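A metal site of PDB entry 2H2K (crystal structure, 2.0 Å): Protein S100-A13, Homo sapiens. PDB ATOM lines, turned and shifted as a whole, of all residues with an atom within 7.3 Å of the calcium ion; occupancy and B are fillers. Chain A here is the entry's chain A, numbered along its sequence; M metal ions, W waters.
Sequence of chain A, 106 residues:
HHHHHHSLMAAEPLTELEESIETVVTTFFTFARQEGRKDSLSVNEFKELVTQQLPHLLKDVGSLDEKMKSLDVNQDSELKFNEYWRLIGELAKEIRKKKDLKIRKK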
ATOM      1  N   PHE A  31      -1.909 -17.767  -1.963  1.00  0.00           N
ATOM      2  CA  PHE A  31      -0.905 -16.952  -2.627  1.00  0.00           C
ATOM      3  C   PHE A  31      -0.445 -15.752  -1.813  1.00  0.00           C
ATOM      4  O   PHE A  31       0.714 -15.348  -1.911  1.00  0.00           O
ATOM      5  CB  PHE A  31      -1.406 -16.500  -3.998  1.00  0.00           C
ATOM      6  CG  PHE A  31      -1.390 -17.587  -5.034  1.00  0.00           C
ATOM      7  CD1 PHE A  31      -2.429 -18.513  -5.112  1.00  0.00           C
ATOM      8  CD2 PHE A  31      -0.302 -17.747  -5.882  1.00  0.00           C
ATOM      9  CE1 PHE A  31      -2.383 -19.577  -6.021  1.00  0.00           C
ATOM     10  CE2 PHE A  31      -0.233 -18.805  -6.794  1.00  0.00           C
ATOM     11  CZ  PHE A  31      -1.288 -19.727  -6.857  1.00  0.00           C
ATOM     12  N   ALA A  32      -1.336 -15.203  -1.006  1.00  0.00           N
ATOM     13  CA  ALA A  32      -1.016 -14.019  -0.201  1.00  0.00           C
ATOM     14  C   ALA A  32      -0.093 -14.275   0.982  1.00  0.00           C
ATOM     15  O   ALA A  32       0.518 -13.334   1.509  1.00  0.00           O
ATOM     16  CB  ALA A  32      -2.317 -13.365   0.285  1.00  0.00           C
ATOM     17  N   ARG A  33       0.032 -15.534   1.401  1.00  0.00           N
ATOM     18  CA  ARG A  33       0.898 -15.874   2.529  1.00  0.00           C
ATOM     19  C   ARG A  33       2.361 -16.115   2.126  1.00  0.00           C
ATOM     20  O   ARG A  33       3.203 -16.336   2.981  1.00  0.00           O
ATOM     21  CB  ARG A  33       0.377 -17.139   3.253  1.00  0.00           C
ATOM     22  CG  ARG A  33      -0.668 -16.929   4.370  1.00  0.00           C
ATOM     23  CD  ARG A  33      -2.052 -16.559   3.838  1.00  0.00           C
ATOM     24  NE  ARG A  33      -3.152 -17.263   4.515  1.00  0.00           N
ATOM     25  CZ  ARG A  33      -3.563 -17.038   5.763  1.00  0.00           C
ATOM     26  NH1 ARG A  33      -2.958 -16.133   6.509  1.00  0.00           N
ATOM     27  NH2 ARG A  33      -4.591 -17.715   6.271  1.00  0.00           N
ATOM     28  N   GLN A  34       2.657 -16.078   0.832  1.00  0.00           N
ATOM     29  CA  GLN A  34       4.034 -16.346   0.388  1.00  0.00           C
ATOM     30  C   GLN A  34       5.087 -15.318   0.824  1.00  0.00           C
ATOM     31  O   GLN A  34       6.210 -15.716   1.153  1.00  0.00           O
ATOM     32  CB  GLN A  34       4.084 -16.533  -1.142  1.00  0.00           C
ATOM     33  CG  GLN A  34       3.259 -17.720  -1.665  1.00  0.00           C
ATOM     34  CD  GLN A  34       3.553 -19.030  -0.927  1.00  0.00           C
ATOM     35  OE1 GLN A  34       2.679 -19.593  -0.269  1.00  0.00           O
ATOM     36  NE2 GLN A  34       4.780 -19.516  -1.054  1.00  0.00           N
ATOM     37  N   GLU A  35       4.754 -14.025   0.829  1.00  0.00           N
ATOM     38  CA  GLU A  35       5.726 -13.004   1.246  1.00  0.00           C
ATOM     39  C   GLU A  35       5.026 -11.798   1.888  1.00  0.00           C
ATOM     40  O   GLU A  35       3.820 -11.600   1.716  1.00  0.00           O
ATOM     41  CB  GLU A  35       6.590 -12.544   0.058  1.00  0.00           C
ATOM     42  CG  GLU A  35       5.956 -11.499  -0.860  1.00  0.00           C
ATOM     43  CD  GLU A  35       6.811 -11.192  -2.085  1.00  0.00           C
ATOM     44  OE1 GLU A  35       7.857 -11.863  -2.267  1.00  0.00           O
ATOM     45  OE2 GLU A  35       6.432 -10.309  -2.885  1.00  0.00           O
ATOM     46  N   GLY A  36       5.779 -11.011   2.652  1.00  0.00           N
ATOM     47  CA  GLY A  36       5.212  -9.838   3.305  1.00  0.00           C
ATOM     48  C   GLY A  36       3.936 -10.086   4.082  1.00  0.00           C
ATOM     49  O   GLY A  36       3.778 -11.127   4.720  1.00  0.00           O
ATOM     50  N   ARG A  37       3.006  -9.126   4.032  1.00  0.00           N
ATOM     51  CA  ARG A  37       1.737  -9.237   4.740  1.00  0.00           C
ATOM     52  C   ARG A  37       1.018 -10.511   4.269  1.00  0.00           C
ATOM     53  O   ARG A  37       0.927 -10.775   3.062  1.00  0.00           O
ATOM     54  CB  ARG A  37       0.856  -8.005   4.457  1.00  0.00           C
ATOM     55  CG  ARG A  37       1.464  -6.627   4.808  1.00  0.00           C
ATOM     56  CD  ARG A  37       1.689  -6.420   6.311  1.00  0.00           C
ATOM     57  NE  ARG A  37       1.781  -4.999   6.664  1.00  0.00           N
ATOM     58  CZ  ARG A  37       2.122  -4.547   7.865  1.00  0.00           C
ATOM     59  NH1 ARG A  37       2.412  -5.404   8.844  1.00  0.00           N
ATOM     60  NH2 ARG A  37       2.166  -3.247   8.098  1.00  0.00           N
ATOM     61  N   LYS A  38       0.525 -11.298   5.220  1.00  0.00           N
ATOM     62  CA  LYS A  38      -0.149 -12.551   4.893  1.00  0.00           C
ATOM     63  C   LYS A  38      -1.588 -12.401   4.412  1.00  0.00           C
ATOM     64  O   LYS A  38      -2.173 -13.356   3.896  1.00  0.00           O
ATOM     65  CB  LYS A  38      -0.109 -13.489   6.110  1.00  0.00           C
ATOM     66  CG  LYS A  38       1.269 -13.621   6.694  1.00  0.00           C
ATOM     67  CD  LYS A  38       1.606 -15.032   7.096  1.00  0.00           C
ATOM     68  CE  LYS A  38       3.107 -15.219   7.162  1.00  0.00           C
ATOM     69  NZ  LYS A  38       3.525 -16.129   6.062  1.00  0.00           N
ATOM     70  N   ASP A  39      -2.163 -11.207   4.575  1.00  0.00           N
ATOM     71  CA  ASP A  39      -3.534 -10.985   4.143  1.00  0.00           C
ATOM     72  C   ASP A  39      -3.668 -10.134   2.880  1.00  0.00           C
ATOM     73  O   ASP A  39      -4.743  -9.600   2.595  1.00  0.00           O
ATOM     74  CB  ASP A  39      -4.352 -10.356   5.290  1.00  0.00           C
ATOM     75  CG  ASP A  39      -3.833  -8.989   5.695  1.00  0.00           C
ATOM     76  OD1 ASP A  39      -2.649  -8.703   5.406  1.00  0.00           O
ATOM     77  OD2 ASP A  39      -4.593  -8.221   6.317  1.00  0.00           O
ATOM     78  N   SER A  40      -2.565 -10.015   2.130  1.00  0.00           N
ATOM     79  CA  SER A  40      -2.551  -9.208   0.918  1.00  0.00           C
ATOM     80  C   SER A  40      -1.576  -9.766  -0.104  1.00  0.00           C
ATOM     81  O   SER A  40      -0.543 -10.318   0.254  1.00  0.00           O
ATOM     82  CB  SER A  40      -2.205  -7.754   1.245  1.00  0.00           C
ATOM     83  OG  SER A  40      -0.804  -7.600   1.423  1.00  0.00           O
ATOM     84  N   LEU A  41      -1.912  -9.623  -1.382  1.00  0.00           N
ATOM     85  CA  LEU A  41      -1.002  -9.989  -2.465  1.00  0.00           C
ATOM     86  C   LEU A  41      -0.058  -8.838  -2.797  1.00  0.00           C
ATOM     87  O   LEU A  41      -0.498  -7.767  -3.235  1.00  0.00           O
ATOM     88  CB  LEU A  41      -1.791 -10.403  -3.701  1.00  0.00           C
ATOM     89  CG  LEU A  41      -2.865 -11.478  -3.504  1.00  0.00           C
ATOM     90  CD1 LEU A  41      -3.904 -11.410  -4.608  1.00  0.00           C
ATOM     91  CD2 LEU A  41      -2.241 -12.860  -3.428  1.00  0.00           C
ATOM     92  N   SER A  42       1.233  -9.060  -2.600  1.00  0.00           N
ATOM     93  CA  SER A  42       2.265  -8.315  -3.309  1.00  0.00           C
ATOM     94  C   SER A  42       2.117  -8.475  -4.821  1.00  0.00           C
ATOM     95  O   SER A  42       1.379  -9.339  -5.300  1.00  0.00           O
ATOM     96  CB  SER A  42       3.662  -8.765  -2.870  1.00  0.00           C
ATOM     97  OG  SER A  42       4.080  -9.905  -3.595  1.00  0.00           O
ATOM     98  N   GLU A  45       3.165 -11.929  -5.852  1.00  0.00           N
ATOM     99  CA  GLU A  45       2.210 -12.963  -5.474  1.00  0.00           C
ATOM    100  C   GLU A  45       1.049 -12.896  -6.463  1.00  0.00           C
ATOM    101  O   GLU A  45       0.500 -13.923  -6.881  1.00  0.00           O
ATOM    102  CB  GLU A  45       1.714 -12.742  -4.043  1.00  0.00           C
ATOM    103  CG  GLU A  45       2.774 -12.927  -2.958  1.00  0.00           C
ATOM    104  CD  GLU A  45       2.276 -12.526  -1.584  1.00  0.00           C
ATOM    105  OE1 GLU A  45       1.452 -11.597  -1.502  1.00  0.00           O
ATOM    106  OE2 GLU A  45       2.739 -13.106  -0.576  1.00  0.00           O
ATOM    107  N   GLU A  78      -0.446  -3.288  -2.623  1.00  0.00           N
ATOM    108  CA  GLU A  78      -0.855  -4.649  -2.296  1.00  0.00           C
ATOM    109  C   GLU A  78      -2.317  -4.836  -2.687  1.00  0.00           C
ATOM    110  O   GLU A  78      -3.063  -3.862  -2.808  1.00  0.00           O
ATOM    111  CB  GLU A  78      -0.745  -4.889  -0.789  1.00  0.00           C
ATOM    112  CG  GLU A  78       0.651  -4.718  -0.184  1.00  0.00           C
ATOM    113  CD  GLU A  78       1.496  -5.969  -0.312  1.00  0.00           C
ATOM    114  OE1 GLU A  78       0.963  -7.067  -0.035  1.00  0.00           O
ATOM    115  OE2 GLU A  78       2.680  -5.850  -0.665  1.00  0.00           O
ATOM    116  N   LEU A  79      -2.723  -6.078  -2.892  1.00  0.00           N
ATOM    117  CA  LEU A  79      -4.118  -6.354  -3.213  1.00  0.00           C
ATOM    118  C   LEU A  79      -4.703  -7.088  -2.013  1.00  0.00           C
ATOM    119  O   LEU A  79      -4.358  -8.244  -1.750  1.00  0.00           O
ATOM    120  CB  LEU A  79      -4.253  -7.223  -4.465  1.00  0.00           C
ATOM    121  CG  LEU A  79      -3.709  -6.694  -5.805  1.00  0.00           C
ATOM    122  CD1 LEU A  79      -4.199  -7.613  -6.926  1.00  0.00           C
ATOM    123  CD2 LEU A  79      -4.207  -5.264  -6.043  1.00  0.00           C
HETATM  124 CA    CA M   1       1.554 -11.321   0.904  1.00  0.00          CA
HETATM  125  O   HOH W   1       2.293  -9.082   0.586  1.00  0.00           O
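The calcium ion is bound by O of Arg 37, 2.3 Å away.
The backbone carbonyl oxygen (O) of Ala 32 binds the calcium ion (2.3 Å).
The calcium ion is bound by water W1 (2.4 Å).
O of Ser 40 binds the calcium ion.
The backbone carbonyl oxygen (O) of Glu 35 binds the calcium ion (2.4 Å).
The calcium ion is bound by OE1 of Glu 45, at 2.4 Å.
OE2 of Glu 45 is bound to the calcium ion (2.6 Å).
Within 4 Å of the calcium ion: Ala 32, Glu 35, Arg 37, Ser 40 and Glu 45.
The nearest printed residue that does not touch the calcium ion is Gly 36 (4.2 Å).
Water W1 lies within hydrogen-bond range of OE1 of Glu 78 (2.5 Å) and N of Ser 42 (3.4 Å).
OG of Ser 42 lies within hydrogen-bond range of OE2 of Glu 35, 2.5 Å away.
N of Glu 45 sits at hydrogen-bond distance from OG of Ser 42, at 3.2 Å.
The side-chain carboxylate (OE2) of Glu 45 sits close to the backbone NH (N) of Gln 34.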
